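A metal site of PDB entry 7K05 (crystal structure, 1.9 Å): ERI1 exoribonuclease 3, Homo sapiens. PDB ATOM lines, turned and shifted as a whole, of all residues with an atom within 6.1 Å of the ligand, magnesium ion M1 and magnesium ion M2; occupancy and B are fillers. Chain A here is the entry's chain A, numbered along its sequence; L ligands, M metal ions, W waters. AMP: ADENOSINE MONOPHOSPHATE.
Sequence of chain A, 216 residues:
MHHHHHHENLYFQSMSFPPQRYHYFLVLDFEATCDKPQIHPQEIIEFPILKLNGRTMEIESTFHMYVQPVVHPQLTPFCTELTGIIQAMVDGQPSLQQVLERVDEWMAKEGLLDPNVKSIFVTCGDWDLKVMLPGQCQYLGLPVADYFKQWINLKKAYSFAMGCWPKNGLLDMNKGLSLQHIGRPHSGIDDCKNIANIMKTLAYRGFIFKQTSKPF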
ATOM      1  N   LEU A  28      34.703  22.597  29.503  1.00  0.00           N
ATOM      2  CA  LEU A  28      34.540  23.801  28.706  1.00  0.00           C
ATOM      3  C   LEU A  28      33.195  23.789  27.986  1.00  0.00           C
ATOM      4  O   LEU A  28      32.754  22.726  27.522  1.00  0.00           O
ATOM      5  CB  LEU A  28      35.707  23.908  27.728  1.00  0.00           C
ATOM      6  CG  LEU A  28      35.692  25.110  26.804  1.00  0.00           C
ATOM      7  CD1 LEU A  28      37.083  25.532  26.451  1.00  0.00           C
ATOM      8  CD2 LEU A  28      35.008  24.633  25.509  1.00  0.00           C
ATOM      9  N   ASP A  29      32.510  24.934  27.902  1.00  0.00           N
ATOM     10  CA  ASP A  29      31.274  24.979  27.122  1.00  0.00           C
ATOM     11  C   ASP A  29      31.023  26.401  26.642  1.00  0.00           C
ATOM     12  O   ASP A  29      30.560  27.233  27.425  1.00  0.00           O
ATOM     13  CB  ASP A  29      30.087  24.475  27.947  1.00  0.00           C
ATOM     14  CG  ASP A  29      28.768  24.474  27.081  1.00  0.00           C
ATOM     15  OD1 ASP A  29      28.502  23.455  26.473  1.00  0.00           O
ATOM     16  OD2 ASP A  29      28.023  25.474  27.004  1.00  0.00           O
ATOM     17  N   PHE A  30      31.336  26.680  25.383  1.00  0.00           N
ATOM     18  CA  PHE A  30      31.226  28.049  24.901  1.00  0.00           C
ATOM     19  C   PHE A  30      29.788  28.478  24.812  1.00  0.00           C
ATOM     20  O   PHE A  30      28.913  27.643  24.520  1.00  0.00           O
ATOM     21  CB  PHE A  30      31.799  28.191  23.476  1.00  0.00           C
ATOM     22  CG  PHE A  30      33.274  27.914  23.361  1.00  0.00           C
ATOM     23  CD1 PHE A  30      34.188  28.579  24.204  1.00  0.00           C
ATOM     24  CD2 PHE A  30      33.758  27.019  22.393  1.00  0.00           C
ATOM     25  CE1 PHE A  30      35.545  28.369  24.109  1.00  0.00           C
ATOM     26  CE2 PHE A  30      35.135  26.756  22.299  1.00  0.00           C
ATOM     27  CZ  PHE A  30      36.050  27.480  23.116  1.00  0.00           C
ATOM     28  N   GLU A  31      29.552  29.796  24.889  1.00  0.00           N
ATOM     29  CA  GLU A  31      28.393  30.357  24.211  1.00  0.00           C
ATOM     30  C   GLU A  31      28.893  31.218  23.052  1.00  0.00           C
ATOM     31  O   GLU A  31      29.992  31.756  23.095  1.00  0.00           O
ATOM     32  CB  GLU A  31      27.513  31.202  25.132  1.00  0.00           C
ATOM     33  CG  GLU A  31      26.961  30.409  26.321  1.00  0.00           C
ATOM     34  CD  GLU A  31      26.239  29.094  25.942  1.00  0.00           C
ATOM     35  OE1 GLU A  31      25.463  29.073  24.950  1.00  0.00           O
ATOM     36  OE2 GLU A  31      26.421  28.105  26.692  1.00  0.00           O
ATOM     37  N   ALA A  32      28.077  31.343  22.009  1.00  0.00           N
ATOM     38  CA  ALA A  32      28.468  32.121  20.837  1.00  0.00           C
ATOM     39  C   ALA A  32      27.322  33.007  20.388  1.00  0.00           C
ATOM     40  O   ALA A  32      26.150  32.720  20.671  1.00  0.00           O
ATOM     41  CB  ALA A  32      28.860  31.170  19.667  1.00  0.00           C
ATOM     42  N   THR A  33      27.658  34.054  19.625  1.00  0.00           N
ATOM     43  CA  THR A  33      26.621  34.832  18.931  1.00  0.00           C
ATOM     44  C   THR A  33      25.744  33.872  18.097  1.00  0.00           C
ATOM     45  O   THR A  33      26.191  32.822  17.640  1.00  0.00           O
ATOM     46  CB  THR A  33      27.221  35.886  18.008  1.00  0.00           C
ATOM     47  OG1 THR A  33      28.114  35.213  17.110  1.00  0.00           O
ATOM     48  CG2 THR A  33      28.046  36.954  18.846  1.00  0.00           C
ATOM     49  N   CYS A  34      24.476  34.201  17.973  1.00  0.00           N
ATOM     50  CA  CYS A  34      23.558  33.346  17.230  1.00  0.00           C
ATOM     51  C   CYS A  34      22.388  34.208  16.819  1.00  0.00           C
ATOM     52  O   CYS A  34      22.289  35.363  17.232  1.00  0.00           O
ATOM     53  CB  CYS A  34      23.055  32.160  18.055  1.00  0.00           C
ATOM     54  SG  CYS A  34      22.539  32.592  19.717  1.00  0.00           S
ATOM     55  N   ASP A  35      21.478  33.599  16.014  1.00  0.00           N
ATOM     56  CA  ASP A  35      20.281  34.269  15.549  1.00  0.00           C
ATOM     57  C   ASP A  35      19.372  33.197  14.942  1.00  0.00           C
ATOM     58  O   ASP A  35      19.750  32.020  14.813  1.00  0.00           O
ATOM     59  CB  ASP A  35      20.622  35.380  14.539  1.00  0.00           C
ATOM     60  CG  ASP A  35      19.514  36.499  14.469  1.00  0.00           C
ATOM     61  OD1 ASP A  35      18.470  36.406  15.180  1.00  0.00           O
ATOM     62  OD2 ASP A  35      19.725  37.498  13.728  1.00  0.00           O
ATOM     63  N   LYS A  36      18.170  33.626  14.546  1.00  0.00           N
ATOM     64  CA  LYS A  36      17.231  32.773  13.785  1.00  0.00           C
ATOM     65  C   LYS A  36      16.980  33.432  12.440  1.00  0.00           C
ATOM     66  O   LYS A  36      16.441  34.555  12.420  1.00  0.00           O
ATOM     67  CB  LYS A  36      15.905  32.605  14.529  1.00  0.00           C
ATOM     68  CG  LYS A  36      15.437  31.162  14.756  1.00  0.00           C
ATOM     69  CD  LYS A  36      16.397  30.437  15.692  1.00  0.00           C
ATOM     70  CE  LYS A  36      16.075  28.975  15.790  1.00  0.00           C
ATOM     71  NZ  LYS A  36      17.239  28.178  16.173  1.00  0.00           N
ATOM     72  N   GLN A  38      20.567  31.101  11.554  1.00  0.00           N
ATOM     73  CA  GLN A  38      21.811  31.259  12.300  1.00  0.00           C
ATOM     74  C   GLN A  38      22.668  32.400  11.742  1.00  0.00           C
ATOM     75  O   GLN A  38      22.736  32.618  10.530  1.00  0.00           O
ATOM     76  CB  GLN A  38      22.583  29.951  12.248  1.00  0.00           C
ATOM     77  CG  GLN A  38      23.787  29.923  13.196  1.00  0.00           C
ATOM     78  CD  GLN A  38      23.357  30.205  14.601  1.00  0.00           C
ATOM     79  OE1 GLN A  38      23.159  31.389  14.951  1.00  0.00           O
ATOM     80  NE2 GLN A  38      23.147  29.143  15.432  1.00  0.00           N
ATOM     81  N   GLN A  42      29.594  32.792  13.439  1.00  0.00           N
ATOM     82  CA  GLN A  42      29.338  32.865  14.877  1.00  0.00           C
ATOM     83  C   GLN A  42      30.633  33.213  15.567  1.00  0.00           C
ATOM     84  O   GLN A  42      31.716  32.934  15.041  1.00  0.00           O
ATOM     85  CB  GLN A  42      28.835  31.535  15.439  1.00  0.00           C
ATOM     86  CG  GLN A  42      27.434  31.072  14.909  1.00  0.00           C
ATOM     87  CD  GLN A  42      27.009  29.796  15.657  1.00  0.00           C
ATOM     88  OE1 GLN A  42      27.311  28.676  15.232  1.00  0.00           O
ATOM     89  NE2 GLN A  42      26.420  29.969  16.833  1.00  0.00           N
ATOM     90  N   ILE A  45      31.282  34.265  22.717  1.00  0.00           N
ATOM     91  CA  ILE A  45      31.027  35.373  23.650  1.00  0.00           C
ATOM     92  C   ILE A  45      31.176  34.967  25.117  1.00  0.00           C
ATOM     93  O   ILE A  45      31.086  35.842  25.987  1.00  0.00           O
ATOM     94  CB  ILE A  45      29.637  36.020  23.412  1.00  0.00           C
ATOM     95  CG1 ILE A  45      28.527  34.945  23.569  1.00  0.00           C
ATOM     96  CG2 ILE A  45      29.552  36.712  22.036  1.00  0.00           C
ATOM     97  CD1 ILE A  45      27.097  35.523  23.380  1.00  0.00           C
ATOM     98  N   PHE A  78      17.539  37.194  19.984  1.00  0.00           N
ATOM     99  CA  PHE A  78      17.561  35.752  20.121  1.00  0.00           C
ATOM    100  C   PHE A  78      18.735  35.295  20.991  1.00  0.00           C
ATOM    101  O   PHE A  78      18.566  34.475  21.902  1.00  0.00           O
ATOM    102  CB  PHE A  78      17.637  35.082  18.755  1.00  0.00           C
ATOM    103  CG  PHE A  78      17.718  33.583  18.877  1.00  0.00           C
ATOM    104  CD1 PHE A  78      16.565  32.855  19.133  1.00  0.00           C
ATOM    105  CD2 PHE A  78      18.928  32.936  18.851  1.00  0.00           C
ATOM    106  CE1 PHE A  78      16.614  31.525  19.300  1.00  0.00           C
ATOM    107  CE2 PHE A  78      19.029  31.577  19.039  1.00  0.00           C
ATOM    108  CZ  PHE A  78      17.844  30.858  19.291  1.00  0.00           C
ATOM    109  N   LEU A  82      18.436  33.314  24.337  1.00  0.00           N
ATOM    110  CA  LEU A  82      18.953  31.954  24.495  1.00  0.00           C
ATOM    111  C   LEU A  82      19.910  31.844  25.681  1.00  0.00           C
ATOM    112  O   LEU A  82      19.723  30.986  26.573  1.00  0.00           O
ATOM    113  CB  LEU A  82      19.667  31.513  23.220  1.00  0.00           C
ATOM    114  CG  LEU A  82      20.109  30.054  23.284  1.00  0.00           C
ATOM    115  CD1 LEU A  82      18.829  29.168  23.115  1.00  0.00           C
ATOM    116  CD2 LEU A  82      21.108  29.854  22.148  1.00  0.00           C
ATOM    117  N   THR A  83      20.900  32.733  25.735  1.00  0.00           N
ATOM    118  CA  THR A  83      22.063  32.573  26.622  1.00  0.00           C
ATOM    119  C   THR A  83      21.973  33.352  27.911  1.00  0.00           C
ATOM    120  O   THR A  83      22.710  33.030  28.848  1.00  0.00           O
ATOM    121  CB  THR A  83      23.352  33.048  25.962  1.00  0.00           C
ATOM    122  OG1 THR A  83      23.269  34.454  25.736  1.00  0.00           O
ATOM    123  CG2 THR A  83      23.625  32.268  24.594  1.00  0.00           C
ATOM    124  N   CYS A 124      30.464  18.951  25.984  1.00  0.00           N
ATOM    125  CA  CYS A 124      29.225  18.243  25.656  1.00  0.00           C
ATOM    126  C   CYS A 124      29.062  18.334  24.131  1.00  0.00           C
ATOM    127  O   CYS A 124      28.638  19.384  23.626  1.00  0.00           O
ATOM    128  CB  CYS A 124      28.047  18.869  26.380  1.00  0.00           C
ATOM    129  SG  CYS A 124      26.479  17.989  26.002  1.00  0.00           S
ATOM    130  N   TRP A 127      31.261  20.032  19.088  1.00  0.00           N
ATOM    131  CA  TRP A 127      31.168  21.334  18.413  1.00  0.00           C
ATOM    132  C   TRP A 127      32.219  22.323  18.910  1.00  0.00           C
ATOM    133  O   TRP A 127      32.826  23.051  18.119  1.00  0.00           O
ATOM    134  CB  TRP A 127      29.783  21.928  18.639  1.00  0.00           C
ATOM    135  CG  TRP A 127      29.539  23.255  17.964  1.00  0.00           C
ATOM    136  CD1 TRP A 127      29.343  23.498  16.597  1.00  0.00           C
ATOM    137  CD2 TRP A 127      29.522  24.519  18.601  1.00  0.00           C
ATOM    138  NE1 TRP A 127      29.194  24.845  16.388  1.00  0.00           N
ATOM    139  CE2 TRP A 127      29.287  25.489  17.606  1.00  0.00           C
ATOM    140  CE3 TRP A 127      29.635  24.912  19.935  1.00  0.00           C
ATOM    141  CZ2 TRP A 127      29.185  26.824  17.904  1.00  0.00           C
ATOM    142  CZ3 TRP A 127      29.547  26.275  20.222  1.00  0.00           C
ATOM    143  CH2 TRP A 127      29.298  27.196  19.202  1.00  0.00           C
ATOM    144  N   ASP A 128      32.384  22.451  20.228  1.00  0.00           N
ATOM    145  CA  ASP A 128      33.222  23.539  20.767  1.00  0.00           C
ATOM    146  C   ASP A 128      34.647  23.514  20.231  1.00  0.00           C
ATOM    147  O   ASP A 128      35.154  24.542  19.773  1.00  0.00           O
ATOM    148  CB  ASP A 128      33.279  23.434  22.296  1.00  0.00           C
ATOM    149  CG  ASP A 128      31.903  23.480  22.912  1.00  0.00           C
ATOM    150  OD1 ASP A 128      31.552  24.496  23.540  1.00  0.00           O
ATOM    151  OD2 ASP A 128      31.119  22.520  22.736  1.00  0.00           O
ATOM    152  N   PRO A 185      20.029  26.500  31.695  1.00  0.00           N
ATOM    153  CA  PRO A 185      20.532  25.951  30.406  1.00  0.00           C
ATOM    154  C   PRO A 185      21.052  27.070  29.502  1.00  0.00           C
ATOM    155  O   PRO A 185      20.526  28.179  29.499  1.00  0.00           O
ATOM    156  CB  PRO A 185      19.292  25.292  29.778  1.00  0.00           C
ATOM    157  CG  PRO A 185      18.410  24.967  31.013  1.00  0.00           C
ATOM    158  CD  PRO A 185      18.622  26.096  31.967  1.00  0.00           C
ATOM    159  N   HIS A 186      22.073  26.757  28.708  1.00  0.00           N
ATOM    160  CA  HIS A 186      22.714  27.704  27.774  1.00  0.00           C
ATOM    161  C   HIS A 186      23.435  28.872  28.427  1.00  0.00           C
ATOM    162  O   HIS A 186      23.824  29.823  27.741  1.00  0.00           O
ATOM    163  CB  HIS A 186      21.719  28.256  26.763  1.00  0.00           C
ATOM    164  CG  HIS A 186      20.913  27.188  26.107  1.00  0.00           C
ATOM    165  ND1 HIS A 186      21.438  26.372  25.134  1.00  0.00           N
ATOM    166  CD2 HIS A 186      19.654  26.737  26.357  1.00  0.00           C
ATOM    167  CE1 HIS A 186      20.521  25.492  24.762  1.00  0.00           C
ATOM    168  NE2 HIS A 186      19.429  25.698  25.491  1.00  0.00           N
ATOM    169  N   SER A 187      23.633  28.835  29.723  1.00  0.00           N
ATOM    170  CA  SER A 187      24.701  29.632  30.337  1.00  0.00           C
ATOM    171  C   SER A 187      25.979  28.788  30.307  1.00  0.00           C
ATOM    172  O   SER A 187      25.976  27.634  30.751  1.00  0.00           O
ATOM    173  CB  SER A 187      24.341  30.015  31.784  1.00  0.00           C
ATOM    174  OG  SER A 187      25.531  30.282  32.548  1.00  0.00           O
ATOM    175  N   GLY A 188      27.074  29.365  29.793  1.00  0.00           N
ATOM    176  CA  GLY A 188      28.284  28.558  29.604  1.00  0.00           C
ATOM    177  C   GLY A 188      28.774  27.956  30.909  1.00  0.00           C
ATOM    178  O   GLY A 188      28.993  26.752  31.020  1.00  0.00           O
ATOM    179  N   ASP A 191      26.392  25.312  32.211  1.00  0.00           N
ATOM    180  CA  ASP A 191      26.559  24.052  31.467  1.00  0.00           C
ATOM    181  C   ASP A 191      27.789  23.306  31.992  1.00  0.00           C
ATOM    182  O   ASP A 191      27.770  22.080  32.159  1.00  0.00           O
ATOM    183  CB  ASP A 191      26.674  24.360  29.971  1.00  0.00           C
ATOM    184  CG  ASP A 191      25.301  24.771  29.320  1.00  0.00           C
ATOM    185  OD1 ASP A 191      24.237  24.610  29.932  1.00  0.00           O
ATOM    186  OD2 ASP A 191      25.299  25.236  28.156  1.00  0.00           O
HETATM  187  P   AMP L   1      24.944  25.425  23.972  1.00  0.00           P
HETATM  188  O1P AMP L   1      26.216  24.901  24.640  1.00  0.00           O
HETATM  189  O2P AMP L   1      24.463  26.653  24.774  1.00  0.00           O
HETATM  190  O3P AMP L   1      23.835  24.439  23.867  1.00  0.00           O
HETATM  191  O5' AMP L   1      25.174  26.011  22.525  1.00  0.00           O
HETATM  192  C5' AMP L   1      26.325  26.730  22.111  1.00  0.00           C
HETATM  193  C4' AMP L   1      25.929  27.803  21.095  1.00  0.00           C
HETATM  194  O4' AMP L   1      25.175  27.211  20.007  1.00  0.00           O
HETATM  195  C3' AMP L   1      25.016  28.892  21.619  1.00  0.00           C
HETATM  196  O3' AMP L   1      25.711  29.923  22.385  1.00  0.00           O
HETATM  197  C2' AMP L   1      24.379  29.436  20.340  1.00  0.00           C
HETATM  198  O2' AMP L   1      25.330  30.251  19.634  1.00  0.00           O
HETATM  199  C1' AMP L   1      24.208  28.129  19.521  1.00  0.00           C
HETATM  200  N9  AMP L   1      22.867  27.535  19.761  1.00  0.00           N
HETATM  201  C8  AMP L   1      22.566  26.635  20.756  1.00  0.00           C
HETATM  202  N7  AMP L   1      21.227  26.298  20.726  1.00  0.00           N
HETATM  203  C5  AMP L   1      20.724  26.965  19.665  1.00  0.00           C
HETATM  204  C6  AMP L   1      19.370  27.082  19.055  1.00  0.00           C
HETATM  205  N6  AMP L   1      18.325  26.391  19.558  1.00  0.00           N
HETATM  206  N1  AMP L   1      19.261  27.903  18.038  1.00  0.00           N
HETATM  207  C2  AMP L   1      20.275  28.634  17.525  1.00  0.00           C
HETATM  208  N3  AMP L   1      21.533  28.589  18.015  1.00  0.00           N
HETATM  209  C4  AMP L   1      21.795  27.781  19.070  1.00  0.00           C
HETATM  210 MG    MG M   1      26.421  26.055  26.610  1.00  0.00          MG
HETATM  211 MG    MG M   2      27.633  23.641  24.437  1.00  0.00          MG
HETATM  212  O   HOH W   1      28.867  25.007  23.580  1.00  0.00           O
HETATM  213  O   HOH W   2      26.542  22.328  25.590  1.00  0.00           O
HETATM  214  O   HOH W   3      28.943  22.206  23.861  1.00  0.00           O
HETATM  215  O   HOH W   4      26.476  23.380  22.677  1.00  0.00           O
HETATM  216  O   HOH W   5      25.324  24.268  20.094  1.00  0.00           O
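NZ of Lys 36 sits at hydrogen-bond distance from N1 of the ligand. The backbone NH (N) of Ala 32 sits at hydrogen-bond distance from an oxygen (O3') of the ligand, 2.8 Å away. The backbone carbonyl oxygen (O) of Ala 32 sits at hydrogen-bond distance from an oxygen (O2') of the ligand. NE2 of Gln 42 is in hydrogen-bond range of O2' of the ligand, at 3.0 Å. A ring nitrogen (ND1) of His 186 sits at hydrogen-bond distance from an oxygen (O2P) of the ligand (3.1 Å). The side-chain amide nitrogen (NE2) of Gln 38 lies within hydrogen-bond range of a nitrogen (N3) of the ligand (3.1 Å). The side-chain sulfur of Cys 34 lies close to an oxygen (O2') of the ligand (3.6 Å). The backbone carbonyl oxygen of Thr 33 sits at hydrogen-bond distance from an oxygen (O2') of the ligand.
OE2 of Glu 31 lies close to N of Gly 188 (3.4 Å). The backbone NH of Ile 45 sits at hydrogen-bond distance from the backbone carbonyl oxygen of Glu 31 (2.8 Å). The side-chain carboxylate of Asp 191 sits at hydrogen-bond distance from the backbone NH of His 186, at 3.3 Å. O of Ala 32 sits at hydrogen-bond distance from SG of Cys 34. NE2 of Gln 42 lies within hydrogen-bond range of O of Thr 33 (3.0 Å). The side-chain amide oxygen (OE1) of Gln 38 is in hydrogen-bond range of the backbone NH (N) of Asp 35 (3.0 Å). The backbone NH (N) of Phe 30 lies within hydrogen-bond range of the side-chain carboxylate (OD1) of Asp 128 (2.9 Å).
Phe 30 touches the ligand (O to C5', 3.7 Å). Phe 78 touches the ligand (CZ to N1, 3.5 Å). Leu 82 touches the ligand (CD2 to C2', 3.8 Å). Thr 83 touches the ligand (CG2 to O3', 3.8 Å). Trp 127 touches the ligand (CZ3 to C5', 3.8 Å).
Residues that only touch magnesium ion M1: Phe 30 (3.6 Å). Within 4 Å of magnesium ion M1: Asp 29, Phe 30, Glu 31 and Asp 191. The nearest printed residue that does not touch magnesium ion M1 is His 186 (4.2 Å).
Of the 23 residues printed, 1 comes within 4 Å of magnesium ion M2. The nearest printed residue that does not touch magnesium ion M2 is Asp 128 (4.04 Å).
Magnesium ion M1 is bound by the side-chain carboxylate (OD2) of Asp 29 (1.7 Å), the side-chain carboxylate (OE2) of Glu 31 (2.1 Å), the side-chain carboxylate (OD2) of Asp 191 (2.1 Å) and an oxygen (O1P) of the ligand (2.3 Å). Slightly farther from magnesium ion M1 lies O2P of the ligand (2.7 Å).
O1P of the ligand is bound to magnesium ion M2 (1.9 Å). Water W3 is bound to magnesium ion M2, 2.0 Å away. Magnesium ion M2 is bound by water W1, 2.0 Å away. Water W2 is bound to magnesium ion M2. Magnesium ion M2 is bound by water W4, at 2.1 Å. OD1 of Asp 29 binds magnesium ion M2, 2.2 Å away.
Water W1 lies within hydrogen-bond range of OD1 of Asp 128 (2.7 Å) and O of Phe 30 (2.8 Å). Water W3 lies within hydrogen-bond range of OD2 of Asp 128 (2.5 Å) and O of Cys 124 (2.8 Å).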
